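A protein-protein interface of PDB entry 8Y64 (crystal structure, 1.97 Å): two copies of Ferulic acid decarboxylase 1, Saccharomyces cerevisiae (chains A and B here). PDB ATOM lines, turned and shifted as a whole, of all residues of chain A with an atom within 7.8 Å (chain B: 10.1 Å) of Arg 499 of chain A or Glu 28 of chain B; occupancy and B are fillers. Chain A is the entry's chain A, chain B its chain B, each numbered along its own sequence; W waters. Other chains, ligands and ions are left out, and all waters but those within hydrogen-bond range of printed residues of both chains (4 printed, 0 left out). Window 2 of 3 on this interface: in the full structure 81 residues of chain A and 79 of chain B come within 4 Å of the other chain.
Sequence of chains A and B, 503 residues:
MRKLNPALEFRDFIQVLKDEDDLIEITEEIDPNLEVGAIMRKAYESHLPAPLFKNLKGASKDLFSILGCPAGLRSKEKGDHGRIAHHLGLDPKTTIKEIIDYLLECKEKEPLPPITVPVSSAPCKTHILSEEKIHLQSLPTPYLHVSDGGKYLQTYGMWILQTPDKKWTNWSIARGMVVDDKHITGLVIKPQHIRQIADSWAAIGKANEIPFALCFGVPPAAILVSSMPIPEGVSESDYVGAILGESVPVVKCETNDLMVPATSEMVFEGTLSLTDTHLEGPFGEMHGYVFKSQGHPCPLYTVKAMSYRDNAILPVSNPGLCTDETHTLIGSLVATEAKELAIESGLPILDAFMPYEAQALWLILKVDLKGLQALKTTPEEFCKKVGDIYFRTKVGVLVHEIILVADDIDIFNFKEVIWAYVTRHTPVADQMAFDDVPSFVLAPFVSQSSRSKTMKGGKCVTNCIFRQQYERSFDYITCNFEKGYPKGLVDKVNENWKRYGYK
No position is printed for both chains.
The side-chain amide oxygen of Asn 494 of chain A is in hydrogen-bond range of the side-chain amino group of Lys 42 of chain B, at 2.9 Å.
OE2 of Glu 28 of chain B is in salt-bridge range of NE of Arg 499 of chain A (3.0 Å).
The side-chain hydroxyl (OH) of Tyr 502 of chain A lies close to the backbone nitrogen (N) of Pro 51 of chain B (3.4 Å).
O of Trp 497 of chain A sits at hydrogen-bond distance from N of Tyr 502 of chain A, 3.3 Å away.
OE2 of Glu 25 of chain B lies within salt-bridge range of NZ of Lys 54 of chain B (3.4 Å).
The backbone NH (N) of Ile 30 of chain B is in hydrogen-bond range of the backbone carbonyl oxygen (O) of Asn 55 of chain B.
The backbone NH of Lys 57 of chain B is in hydrogen-bond range of the backbone carbonyl oxygen of Ile 30 of chain B (2.9 Å).
N of Asp 31 of chain B lies within hydrogen-bond range of OE2 of Glu 35 of chain B (2.9 Å).
Water W2 lies within hydrogen-bond range of OH of Tyr 500 of chain A (2.6 Å) and OE1 of Glu 35 of chain B (2.6 Å).
Water W3 bridges OE2 of Glu 28 of chain B (2.6 Å) and NH2 of Arg 499 of chain A (3.0 Å).
Water W4 lies within hydrogen-bond range of the backbone NH of Thr 27 of chain B (2.8 Å), the backbone carbonyl oxygen of Tyr 500 of chain A (2.8 Å) and the backbone NH of Glu 28 of chain B (3.4 Å).
Val 493 of chain A touches Ile 39 of chain B (CG2 to CG1, 3.99 Å).
Ile 39 of chain B touches Trp 497 of chain A.
Trp 497 of chain A touches Lys 42 of chain B.
Tyr 500 of chain A touches Ile 24 of chain B.
Tyr 500 of chain A touches Glu 25 of chain B (O to O, 3.8 Å).
CD1 of Ile 30 of chain B touches CE1 of Tyr 500 of chain A, at 3.7 Å.
Glu 35 of chain B touches Tyr 500 of chain A (OE1 to OH, 3.6 Å).
Tyr 500 of chain A touches Ile 39 of chain B.
Gly 501 of chain A touches Ile 24 of chain B.
CG1 of Ile 24 of chain B touches CE1 of Tyr 502 of chain A, 3.6 Å away.
No residue of chain B comes within 4 Å of Asn 496 of chain A.
Of chain B, only Glu 28 comes within 4 Å of Arg 499 of chain A.
Of the printed residues of chain A, Glu 25 of chain B touches Tyr 500 (3.8 Å).
Glu 28 of chain B touches just one residue of chain A: Arg 499.
Of the printed residues of chain A, Ile 30 of chain B touches Tyr 500.
Pro 32 of chain B touches none of the printed residues of chain A.
Phe 53 of chain B touches none of the printed residues of chain A.
The nearest residue of chain A that does not touch Glu 28 of chain B is Tyr 500 of chain A (4.03 Å).
The nearest printed residue of chain A that does not touch Ile 39 of chain B is Tyr 502 of chain A (4.9 Å).
Hydrophobic or aromatic side chains of chain A that line the printed part of chain B: Val 493, Trp 497, Tyr 500 and Tyr 502.
Printed residues of chain B that touch a printed residue of chain A: Ile 24, Glu 25, Glu 28, Ile 30, Glu 35, Ile 39, Lys 42 and Pro 51.
Along chain B the printed residues that touch a printed residue of chain A span positions 24 to 51.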
ATOM      1  N   VAL A 493      -9.104  -8.912  -7.904  1.00  0.00           N
ATOM      2  CA  VAL A 493      -9.527  -9.799  -8.990  1.00  0.00           C
ATOM      3  C   VAL A 493      -8.829 -11.157  -8.883  1.00  0.00           C
ATOM      4  O   VAL A 493      -9.457 -12.216  -9.027  1.00  0.00           O
ATOM      5  CB  VAL A 493      -9.264  -9.128 -10.348  1.00  0.00           C
ATOM      6  CG1 VAL A 493      -9.399 -10.155 -11.504  1.00  0.00           C
ATOM      7  CG2 VAL A 493     -10.239  -7.942 -10.548  1.00  0.00           C
ATOM      8  N   ASN A 494      -7.518 -11.147  -8.636  1.00  0.00           N
ATOM      9  CA  ASN A 494      -6.809 -12.413  -8.490  1.00  0.00           C
ATOM     10  C   ASN A 494      -7.326 -13.193  -7.290  1.00  0.00           C
ATOM     11  O   ASN A 494      -7.484 -14.416  -7.356  1.00  0.00           O
ATOM     12  CB  ASN A 494      -5.309 -12.175  -8.381  1.00  0.00           C
ATOM     13  CG  ASN A 494      -4.691 -11.860  -9.710  1.00  0.00           C
ATOM     14  OD1 ASN A 494      -5.226 -12.258 -10.741  1.00  0.00           O
ATOM     15  ND2 ASN A 494      -3.558 -11.156  -9.707  1.00  0.00           N
ATOM     16  N   GLU A 495      -7.628 -12.495  -6.198  1.00  0.00           N
ATOM     17  CA  GLU A 495      -8.059 -13.159  -4.971  1.00  0.00           C
ATOM     18  C   GLU A 495      -9.451 -13.760  -5.120  1.00  0.00           C
ATOM     19  O   GLU A 495      -9.757 -14.787  -4.498  1.00  0.00           O
ATOM     20  CB  GLU A 495      -8.013 -12.145  -3.818  1.00  0.00           C
ATOM     21  CG  GLU A 495      -8.657 -12.567  -2.520  1.00  0.00           C
ATOM     22  CD  GLU A 495      -8.460 -11.519  -1.411  1.00  0.00           C
ATOM     23  OE1 GLU A 495      -9.075 -10.424  -1.478  1.00  0.00           O
ATOM     24  OE2 GLU A 495      -7.663 -11.782  -0.486  1.00  0.00           O
ATOM     25  N   ASN A 496     -10.298 -13.149  -5.945  1.00  0.00           N
ATOM     26  CA  ASN A 496     -11.670 -13.595  -6.143  1.00  0.00           C
ATOM     27  C   ASN A 496     -11.867 -14.432  -7.401  1.00  0.00           C
ATOM     28  O   ASN A 496     -12.997 -14.850  -7.669  1.00  0.00           O
ATOM     29  CB  ASN A 496     -12.611 -12.384  -6.171  1.00  0.00           C
ATOM     30  CG  ASN A 496     -12.765 -11.739  -4.792  1.00  0.00           C
ATOM     31  OD1 ASN A 496     -13.103 -12.409  -3.823  1.00  0.00           O
ATOM     32  ND2 ASN A 496     -12.519 -10.451  -4.709  1.00  0.00           N
ATOM     33  N   TRP A 497     -10.803 -14.696  -8.161  1.00  0.00           N
ATOM     34  CA  TRP A 497     -10.929 -15.344  -9.467  1.00  0.00           C
ATOM     35  C   TRP A 497     -11.712 -16.657  -9.383  1.00  0.00           C
ATOM     36  O   TRP A 497     -12.643 -16.892 -10.164  1.00  0.00           O
ATOM     37  CB  TRP A 497      -9.532 -15.584 -10.052  1.00  0.00           C
ATOM     38  CG  TRP A 497      -9.533 -15.787 -11.529  1.00  0.00           C
ATOM     39  CD1 TRP A 497      -9.090 -16.897 -12.214  1.00  0.00           C
ATOM     40  CD2 TRP A 497      -9.983 -14.859 -12.513  1.00  0.00           C
ATOM     41  NE1 TRP A 497      -9.251 -16.705 -13.572  1.00  0.00           N
ATOM     42  CE2 TRP A 497      -9.797 -15.463 -13.781  1.00  0.00           C
ATOM     43  CE3 TRP A 497     -10.534 -13.570 -12.452  1.00  0.00           C
ATOM     44  CZ2 TRP A 497     -10.139 -14.821 -14.973  1.00  0.00           C
ATOM     45  CZ3 TRP A 497     -10.884 -12.934 -13.642  1.00  0.00           C
ATOM     46  CH2 TRP A 497     -10.688 -13.559 -14.883  1.00  0.00           C
ATOM     47  N   LYS A 498     -11.365 -17.525  -8.424  1.00  0.00           N
ATOM     48  CA  LYS A 498     -12.077 -18.803  -8.328  1.00  0.00           C
ATOM     49  C   LYS A 498     -13.496 -18.616  -7.793  1.00  0.00           C
ATOM     50  O   LYS A 498     -14.426 -19.310  -8.210  1.00  0.00           O
ATOM     51  CB  LYS A 498     -11.293 -19.764  -7.440  1.00  0.00           C
ATOM     52  CG  LYS A 498      -9.966 -20.177  -8.040  1.00  0.00           C
ATOM     53  CD  LYS A 498      -9.158 -21.007  -7.054  1.00  0.00           C
ATOM     54  CE  LYS A 498      -7.985 -21.674  -7.746  1.00  0.00           C
ATOM     55  NZ  LYS A 498      -6.691 -21.249  -7.159  1.00  0.00           N
ATOM     56  N   ARG A 499     -13.675 -17.695  -6.852  1.00  0.00           N
ATOM     57  CA  ARG A 499     -15.013 -17.375  -6.366  1.00  0.00           C
ATOM     58  C   ARG A 499     -15.932 -16.922  -7.503  1.00  0.00           C
ATOM     59  O   ARG A 499     -17.136 -17.215  -7.498  1.00  0.00           O
ATOM     60  CB  ARG A 499     -14.906 -16.301  -5.283  1.00  0.00           C
ATOM     61  CG  ARG A 499     -16.206 -15.966  -4.579  1.00  0.00           C
ATOM     62  CD  ARG A 499     -15.971 -14.790  -3.628  1.00  0.00           C
ATOM     63  NE  ARG A 499     -17.111 -14.580  -2.753  1.00  0.00           N
ATOM     64  CZ  ARG A 499     -17.244 -15.148  -1.561  1.00  0.00           C
ATOM     65  NH1 ARG A 499     -16.286 -15.900  -1.042  1.00  0.00           N
ATOM     66  NH2 ARG A 499     -18.362 -14.946  -0.869  1.00  0.00           N
ATOM     67  N   TYR A 500     -15.389 -16.208  -8.492  1.00  0.00           N
ATOM     68  CA  TYR A 500     -16.209 -15.842  -9.648  1.00  0.00           C
ATOM     69  C   TYR A 500     -16.730 -17.070 -10.375  1.00  0.00           C
ATOM     70  O   TYR A 500     -17.827 -17.040 -10.951  1.00  0.00           O
ATOM     71  CB  TYR A 500     -15.410 -14.996 -10.634  1.00  0.00           C
ATOM     72  CG  TYR A 500     -14.907 -13.673 -10.119  1.00  0.00           C
ATOM     73  CD1 TYR A 500     -15.544 -13.002  -9.079  1.00  0.00           C
ATOM     74  CD2 TYR A 500     -13.791 -13.084 -10.702  1.00  0.00           C
ATOM     75  CE1 TYR A 500     -15.057 -11.768  -8.627  1.00  0.00           C
ATOM     76  CE2 TYR A 500     -13.302 -11.867 -10.268  1.00  0.00           C
ATOM     77  CZ  TYR A 500     -13.935 -11.211  -9.244  1.00  0.00           C
ATOM     78  OH  TYR A 500     -13.415 -10.002  -8.845  1.00  0.00           O
ATOM     79  N   GLY A 501     -15.935 -18.136 -10.413  1.00  0.00           N
ATOM     80  CA  GLY A 501     -16.287 -19.323 -11.159  1.00  0.00           C
ATOM     81  C   GLY A 501     -15.188 -19.829 -12.075  1.00  0.00           C
ATOM     82  O   GLY A 501     -15.356 -20.874 -12.698  1.00  0.00           O
ATOM     83  N   TYR A 502     -14.070 -19.108 -12.174  1.00  0.00           N
ATOM     84  CA  TYR A 502     -12.966 -19.520 -13.031  1.00  0.00           C
ATOM     85  C   TYR A 502     -12.127 -20.599 -12.359  1.00  0.00           C
ATOM     86  O   TYR A 502     -12.174 -20.798 -11.145  1.00  0.00           O
ATOM     87  CB  TYR A 502     -12.049 -18.339 -13.361  1.00  0.00           C
ATOM     88  CG  TYR A 502     -12.592 -17.452 -14.447  1.00  0.00           C
ATOM     89  CD1 TYR A 502     -12.340 -17.726 -15.783  1.00  0.00           C
ATOM     90  CD2 TYR A 502     -13.355 -16.327 -14.133  1.00  0.00           C
ATOM     91  CE1 TYR A 502     -12.856 -16.907 -16.795  1.00  0.00           C
ATOM     92  CE2 TYR A 502     -13.876 -15.508 -15.131  1.00  0.00           C
ATOM     93  CZ  TYR A 502     -13.616 -15.800 -16.462  1.00  0.00           C
ATOM     94  OH  TYR A 502     -14.113 -14.985 -17.476  1.00  0.00           O
ATOM     95  N   LYS A 503     -11.350 -21.297 -13.173  1.00  0.00           N
ATOM     96  CA  LYS A 503     -10.418 -22.290 -12.671  1.00  0.00           C
ATOM     97  C   LYS A 503      -9.255 -21.607 -11.955  1.00  0.00           C
ATOM     98  O   LYS A 503      -8.811 -22.082 -10.911  1.00  0.00           O
ATOM     99  CB  LYS A 503      -9.910 -23.165 -13.819  1.00  0.00           C
ATOM    100  CG  LYS A 503      -8.698 -24.011 -13.461  1.00  0.00           C
ATOM    101  CD  LYS A 503      -8.235 -24.824 -14.656  1.00  0.00           C
ATOM    102  CE  LYS A 503      -7.358 -25.986 -14.208  1.00  0.00           C
ATOM    103  NZ  LYS A 503      -7.554 -27.197 -15.060  1.00  0.00           N
ATOM    104  N   ILE B  24     -18.330 -18.033 -18.132  1.00  0.00           N
ATOM    105  CA  ILE B  24     -18.512 -18.033 -16.678  1.00  0.00           C
ATOM    106  C   ILE B  24     -19.591 -17.015 -16.345  1.00  0.00           C
ATOM    107  O   ILE B  24     -19.463 -15.837 -16.697  1.00  0.00           O
ATOM    108  CB  ILE B  24     -17.214 -17.694 -15.923  1.00  0.00           C
ATOM    109  CG1 ILE B  24     -16.044 -18.560 -16.402  1.00  0.00           C
ATOM    110  CG2 ILE B  24     -17.443 -17.775 -14.408  1.00  0.00           C
ATOM    111  CD1 ILE B  24     -16.116 -20.013 -16.034  1.00  0.00           C
ATOM    112  N   GLU B  25     -20.648 -17.452 -15.659  1.00  0.00           N
ATOM    113  CA  GLU B  25     -21.677 -16.531 -15.178  1.00  0.00           C
ATOM    114  C   GLU B  25     -21.231 -16.024 -13.814  1.00  0.00           C
ATOM    115  O   GLU B  25     -21.162 -16.788 -12.845  1.00  0.00           O
ATOM    116  CB  GLU B  25     -23.042 -17.208 -15.101  1.00  0.00           C
ATOM    117  CG  GLU B  25     -23.518 -17.738 -16.429  1.00  0.00           C
ATOM    118  CD  GLU B  25     -24.949 -18.226 -16.366  1.00  0.00           C
ATOM    119  OE1 GLU B  25     -25.247 -19.085 -15.503  1.00  0.00           O
ATOM    120  OE2 GLU B  25     -25.767 -17.758 -17.190  1.00  0.00           O
ATOM    121  N   ILE B  26     -20.869 -14.751 -13.750  1.00  0.00           N
ATOM    122  CA  ILE B  26     -20.389 -14.149 -12.514  1.00  0.00           C
ATOM    123  C   ILE B  26     -21.598 -13.536 -11.813  1.00  0.00           C
ATOM    124  O   ILE B  26     -22.217 -12.601 -12.328  1.00  0.00           O
ATOM    125  CB  ILE B  26     -19.293 -13.117 -12.793  1.00  0.00           C
ATOM    126  CG1 ILE B  26     -18.186 -13.748 -13.652  1.00  0.00           C
ATOM    127  CG2 ILE B  26     -18.734 -12.518 -11.485  1.00  0.00           C
ATOM    128  CD1 ILE B  26     -16.932 -12.850 -13.776  1.00  0.00           C
ATOM    129  N   THR B  27     -21.973 -14.112 -10.667  1.00  0.00           N
ATOM    130  CA  THR B  27     -23.067 -13.597  -9.855  1.00  0.00           C
ATOM    131  C   THR B  27     -22.569 -12.820  -8.646  1.00  0.00           C
ATOM    132  O   THR B  27     -23.386 -12.233  -7.930  1.00  0.00           O
ATOM    133  CB  THR B  27     -23.981 -14.733  -9.366  1.00  0.00           C
ATOM    134  OG1 THR B  27     -23.209 -15.657  -8.589  1.00  0.00           O
ATOM    135  CG2 THR B  27     -24.601 -15.468 -10.547  1.00  0.00           C
ATOM    136  N   GLU B  28     -21.261 -12.812  -8.388  1.00  0.00           N
ATOM    137  CA  GLU B  28     -20.714 -11.841  -7.448  1.00  0.00           C
ATOM    138  C   GLU B  28     -20.980 -10.434  -7.977  1.00  0.00           C
ATOM    139  O   GLU B  28     -21.048 -10.211  -9.187  1.00  0.00           O
ATOM    140  CB  GLU B  28     -19.208 -12.054  -7.268  1.00  0.00           C
ATOM    141  CG  GLU B  28     -18.815 -13.448  -6.768  1.00  0.00           C
ATOM    142  CD  GLU B  28     -19.331 -13.728  -5.367  1.00  0.00           C
ATOM    143  OE1 GLU B  28     -20.041 -14.742  -5.180  1.00  0.00           O
ATOM    144  OE2 GLU B  28     -18.998 -12.948  -4.450  1.00  0.00           O
ATOM    145  N   GLU B  29     -21.143  -9.479  -7.064  1.00  0.00           N
ATOM    146  CA  GLU B  29     -21.291  -8.091  -7.479  1.00  0.00           C
ATOM    147  C   GLU B  29     -19.978  -7.561  -8.040  1.00  0.00           C
ATOM    148  O   GLU B  29     -18.941  -7.631  -7.382  1.00  0.00           O
ATOM    149  CB  GLU B  29     -21.726  -7.214  -6.317  1.00  0.00           C
ATOM    150  CG  GLU B  29     -22.036  -5.808  -6.783  1.00  0.00           C
ATOM    151  CD  GLU B  29     -22.358  -4.879  -5.621  1.00  0.00           C
ATOM    152  OE1 GLU B  29     -23.537  -4.844  -5.195  1.00  0.00           O
ATOM    153  OE2 GLU B  29     -21.434  -4.168  -5.163  1.00  0.00           O
ATOM    154  N   ILE B  30     -20.026  -7.015  -9.254  1.00  0.00           N
ATOM    155  CA  ILE B  30     -18.843  -6.494  -9.934  1.00  0.00           C
ATOM    156  C   ILE B  30     -19.071  -5.030 -10.271  1.00  0.00           C
ATOM    157  O   ILE B  30     -20.152  -4.653 -10.730  1.00  0.00           O
ATOM    158  CB  ILE B  30     -18.539  -7.310 -11.206  1.00  0.00           C
ATOM    159  CG1 ILE B  30     -18.193  -8.756 -10.855  1.00  0.00           C
ATOM    160  CG2 ILE B  30     -17.448  -6.629 -12.056  1.00  0.00           C
ATOM    161  CD1 ILE B  30     -16.904  -8.894 -10.020  1.00  0.00           C
ATOM    162  N   ASP B  31     -18.039  -4.209 -10.077  1.00  0.00           N
ATOM    163  CA  ASP B  31     -18.148  -2.772 -10.335  1.00  0.00           C
ATOM    164  C   ASP B  31     -17.898  -2.463 -11.809  1.00  0.00           C
ATOM    165  O   ASP B  31     -16.815  -2.775 -12.320  1.00  0.00           O
ATOM    166  CB  ASP B  31     -17.137  -2.005  -9.479  1.00  0.00           C
ATOM    167  CG  ASP B  31     -17.513  -0.548  -9.297  1.00  0.00           C
ATOM    168  OD1 ASP B  31     -18.248   0.002 -10.151  1.00  0.00           O
ATOM    169  OD2 ASP B  31     -17.046   0.057  -8.310  1.00  0.00           O
ATOM    170  N   PRO B  32     -18.843  -1.827 -12.511  1.00  0.00           N
ATOM    171  CA  PRO B  32     -18.561  -1.342 -13.879  1.00  0.00           C
ATOM    172  C   PRO B  32     -17.394  -0.383 -13.937  1.00  0.00           C
ATOM    173  O   PRO B  32     -16.804  -0.199 -15.016  1.00  0.00           O
ATOM    174  CB  PRO B  32     -19.863  -0.620 -14.273  1.00  0.00           C
ATOM    175  CG  PRO B  32     -20.908  -1.219 -13.379  1.00  0.00           C
ATOM    176  CD  PRO B  32     -20.199  -1.462 -12.073  1.00  0.00           C
ATOM    177  N   GLU B  35     -13.498  -2.582 -12.713  1.00  0.00           N
ATOM    178  CA  GLU B  35     -13.434  -4.010 -12.374  1.00  0.00           C
ATOM    179  C   GLU B  35     -13.843  -4.903 -13.545  1.00  0.00           C
ATOM    180  O   GLU B  35     -13.202  -5.939 -13.802  1.00  0.00           O
ATOM    181  CB  GLU B  35     -14.298  -4.306 -11.142  1.00  0.00           C
ATOM    182  CG  GLU B  35     -14.004  -5.645 -10.487  1.00  0.00           C
ATOM    183  CD  GLU B  35     -14.622  -5.787  -9.087  1.00  0.00           C
ATOM    184  OE1 GLU B  35     -14.001  -6.498  -8.245  1.00  0.00           O
ATOM    185  OE2 GLU B  35     -15.669  -5.166  -8.814  1.00  0.00           O
ATOM    186  N   VAL B  36     -14.922  -4.546 -14.246  1.00  0.00           N
ATOM    187  CA  VAL B  36     -15.311  -5.280 -15.451  1.00  0.00           C
ATOM    188  C   VAL B  36     -14.150  -5.330 -16.435  1.00  0.00           C
ATOM    189  O   VAL B  36     -13.797  -6.396 -16.959  1.00  0.00           O
ATOM    190  CB  VAL B  36     -16.558  -4.643 -16.088  1.00  0.00           C
ATOM    191  CG1 VAL B  36     -16.756  -5.190 -17.485  1.00  0.00           C
ATOM    192  CG2 VAL B  36     -17.803  -4.936 -15.239  1.00  0.00           C
ATOM    193  N   ILE B  39     -11.273  -7.597 -15.169  1.00  0.00           N
ATOM    194  CA  ILE B  39     -11.639  -9.003 -15.300  1.00  0.00           C
ATOM    195  C   ILE B  39     -11.556  -9.433 -16.759  1.00  0.00           C
ATOM    196  O   ILE B  39     -11.007 -10.500 -17.074  1.00  0.00           O
ATOM    197  CB  ILE B  39     -13.039  -9.252 -14.700  1.00  0.00           C
ATOM    198  CG1 ILE B  39     -12.941  -9.240 -13.174  1.00  0.00           C
ATOM    199  CG2 ILE B  39     -13.605 -10.595 -15.168  1.00  0.00           C
ATOM    200  CD1 ILE B  39     -14.263  -8.965 -12.475  1.00  0.00           C
ATOM    201  N   LYS B  42      -7.845  -9.916 -17.811  1.00  0.00           N
ATOM    202  CA  LYS B  42      -7.285 -11.184 -17.327  1.00  0.00           C
ATOM    203  C   LYS B  42      -7.723 -12.350 -18.206  1.00  0.00           C
ATOM    204  O   LYS B  42      -6.910 -13.211 -18.556  1.00  0.00           O
ATOM    205  CB  LYS B  42      -7.691 -11.450 -15.870  1.00  0.00           C
ATOM    206  CG  LYS B  42      -6.927 -12.622 -15.226  1.00  0.00           C
ATOM    207  CD  LYS B  42      -7.242 -12.784 -13.733  1.00  0.00           C
ATOM    208  CE  LYS B  42      -6.735 -14.116 -13.162  1.00  0.00           C
ATOM    209  NZ  LYS B  42      -5.250 -14.108 -12.946  1.00  0.00           N
ATOM    210  N   PRO B  51     -16.440 -13.874 -19.616  1.00  0.00           N
ATOM    211  CA  PRO B  51     -17.218 -13.520 -18.416  1.00  0.00           C
ATOM    212  C   PRO B  51     -18.569 -12.938 -18.804  1.00  0.00           C
ATOM    213  O   PRO B  51     -18.654 -12.017 -19.618  1.00  0.00           O
ATOM    214  CB  PRO B  51     -16.349 -12.465 -17.727  1.00  0.00           C
ATOM    215  CG  PRO B  51     -15.646 -11.768 -18.899  1.00  0.00           C
ATOM    216  CD  PRO B  51     -15.408 -12.865 -19.929  1.00  0.00           C
ATOM    217  N   LEU B  52     -19.628 -13.472 -18.208  1.00  0.00           N
ATOM    218  CA  LEU B  52     -20.953 -12.886 -18.302  1.00  0.00           C
ATOM    219  C   LEU B  52     -21.263 -12.325 -16.918  1.00  0.00           C
ATOM    220  O   LEU B  52     -21.546 -13.086 -15.981  1.00  0.00           O
ATOM    221  CB  LEU B  52     -21.984 -13.919 -18.745  1.00  0.00           C
ATOM    222  CG  LEU B  52     -23.416 -13.393 -18.827  1.00  0.00           C
ATOM    223  CD1 LEU B  52     -23.575 -12.280 -19.869  1.00  0.00           C
ATOM    224  CD2 LEU B  52     -24.382 -14.545 -19.111  1.00  0.00           C
ATOM    225  N   PHE B  53     -21.188 -10.994 -16.788  1.00  0.00           N
ATOM    226  CA  PHE B  53     -21.433 -10.336 -15.509  1.00  0.00           C
ATOM    227  C   PHE B  53     -22.940 -10.202 -15.321  1.00  0.00           C
ATOM    228  O   PHE B  53     -23.585  -9.413 -16.021  1.00  0.00           O
ATOM    229  CB  PHE B  53     -20.756  -8.964 -15.439  1.00  0.00           C
ATOM    230  CG  PHE B  53     -19.284  -8.962 -15.805  1.00  0.00           C
ATOM    231  CD1 PHE B  53     -18.867  -8.794 -17.121  1.00  0.00           C
ATOM    232  CD2 PHE B  53     -18.325  -9.127 -14.818  1.00  0.00           C
ATOM    233  CE1 PHE B  53     -17.518  -8.778 -17.455  1.00  0.00           C
ATOM    234  CE2 PHE B  53     -16.962  -9.128 -15.122  1.00  0.00           C
ATOM    235  CZ  PHE B  53     -16.553  -8.949 -16.444  1.00  0.00           C
ATOM    236  N   LYS B  54     -23.502 -10.964 -14.376  1.00  0.00           N
ATOM    237  CA  LYS B  54     -24.938 -10.964 -14.116  1.00  0.00           C
ATOM    238  C   LYS B  54     -25.347 -10.060 -12.958  1.00  0.00           C
ATOM    239  O   LYS B  54     -26.545  -9.918 -12.705  1.00  0.00           O
ATOM    240  CB  LYS B  54     -25.428 -12.390 -13.818  1.00  0.00           C
ATOM    241  CG  LYS B  54     -25.298 -13.366 -14.997  1.00  0.00           C
ATOM    242  CD  LYS B  54     -26.530 -13.387 -15.883  1.00  0.00           C
ATOM    243  CE  LYS B  54     -27.212 -14.757 -15.855  1.00  0.00           C
ATOM    244  NZ  LYS B  54     -27.857 -15.106 -17.165  1.00  0.00           N
ATOM    245  N   ASN B  55     -24.394  -9.448 -12.246  1.00  0.00           N
ATOM    246  CA  ASN B  55     -24.684  -8.698 -11.031  1.00  0.00           C
ATOM    247  C   ASN B  55     -23.796  -7.458 -10.984  1.00  0.00           C
ATOM    248  O   ASN B  55     -22.904  -7.335 -10.149  1.00  0.00           O
ATOM    249  CB  ASN B  55     -24.478  -9.552  -9.777  1.00  0.00           C
ATOM    250  CG  ASN B  55     -24.884  -8.824  -8.498  1.00  0.00           C
ATOM    251  OD1 ASN B  55     -25.536  -7.777  -8.541  1.00  0.00           O
ATOM    252  ND2 ASN B  55     -24.526  -9.395  -7.354  1.00  0.00           N
ATOM    253  N   LEU B  56     -24.042  -6.526 -11.895  1.00  0.00           N
ATOM    254  CA  LEU B  56     -23.262  -5.297 -11.932  1.00  0.00           C
ATOM    255  C   LEU B  56     -23.778  -4.334 -10.876  1.00  0.00           C
ATOM    256  O   LEU B  56     -24.989  -4.147 -10.732  1.00  0.00           O
ATOM    257  CB  LEU B  56     -23.369  -4.650 -13.306  1.00  0.00           C
ATOM    258  CG  LEU B  56     -22.693  -5.445 -14.418  1.00  0.00           C
ATOM    259  CD1 LEU B  56     -22.995  -4.780 -15.746  1.00  0.00           C
ATOM    260  CD2 LEU B  56     -21.194  -5.575 -14.179  1.00  0.00           C
ATOM    261  N   LYS B  57     -22.853  -3.715 -10.146  1.00  0.00           N
ATOM    262  CA  LYS B  57     -23.204  -2.650  -9.217  1.00  0.00           C
ATOM    263  C   LYS B  57     -23.985  -1.559  -9.929  1.00  0.00           C
ATOM    264  O   LYS B  57     -23.494  -0.969 -10.899  1.00  0.00           O
ATOM    265  CB  LYS B  57     -21.933  -2.056  -8.603  1.00  0.00           C
ATOM    266  CG  LYS B  57     -22.169  -1.328  -7.307  1.00  0.00           C
ATOM    267  CD  LYS B  57     -20.857  -1.154  -6.568  1.00  0.00           C
ATOM    268  CE  LYS B  57     -20.391   0.278  -6.663  1.00  0.00           C
ATOM    269  NZ  LYS B  57     -21.181   1.119  -5.717  1.00  0.00           N
ATOM    270  N   GLY B  58     -25.200  -1.284  -9.441  1.00  0.00           N
ATOM    271  CA  GLY B  58     -26.031  -0.232  -9.990  1.00  0.00           C
ATOM    272  C   GLY B  58     -27.018  -0.667 -11.056  1.00  0.00           C
ATOM    273  O   GLY B  58     -27.864   0.139 -11.461  1.00  0.00           O
ATOM    274  N   ALA B  59     -26.949  -1.909 -11.521  1.00  0.00           N
ATOM    275  CA  ALA B  59     -27.849  -2.364 -12.570  1.00  0.00           C
ATOM    276  C   ALA B  59     -29.272  -2.554 -12.030  1.00  0.00           C
ATOM    277  O   ALA B  59     -29.495  -2.744 -10.834  1.00  0.00           O
ATOM    278  CB  ALA B  59     -27.341  -3.676 -13.169  1.00  0.00           C
ATOM    279  N   SER B  65     -26.960  -6.875 -17.942  1.00  0.00           N
ATOM    280  CA  SER B  65     -25.772  -7.692 -17.818  1.00  0.00           C
ATOM    281  C   SER B  65     -24.739  -7.242 -18.849  1.00  0.00           C
ATOM    282  O   SER B  65     -25.037  -6.473 -19.771  1.00  0.00           O
ATOM    283  CB  SER B  65     -26.112  -9.174 -18.022  1.00  0.00           C
ATOM    284  OG  SER B  65     -26.967  -9.645 -17.003  1.00  0.00           O
ATOM    285  N   ILE B  66     -23.509  -7.737 -18.699  1.00  0.00           N
ATOM    286  CA  ILE B  66     -22.447  -7.483 -19.665  1.00  0.00           C
ATOM    287  C   ILE B  66     -21.833  -8.814 -20.061  1.00  0.00           C
ATOM    288  O   ILE B  66     -21.463  -9.611 -19.193  1.00  0.00           O
ATOM    289  CB  ILE B  66     -21.360  -6.543 -19.108  1.00  0.00           C
ATOM    290  CG1 ILE B  66     -21.811  -5.076 -19.192  1.00  0.00           C
ATOM    291  CG2 ILE B  66     -20.054  -6.730 -19.901  1.00  0.00           C
ATOM    292  CD1 ILE B  66     -20.800  -4.097 -18.574  1.00  0.00           C
HETATM  293  O   HOH W   1     -19.703 -16.998  -6.888  1.00  0.00           O
HETATM  294  O   HOH W   2     -14.708  -8.696  -7.067  1.00  0.00           O
HETATM  295  O   HOH W   3     -20.177 -12.859  -2.135  1.00  0.00           O
HETATM  296  O   HOH W   4     -19.934 -15.735  -9.647  1.00  0.00           O
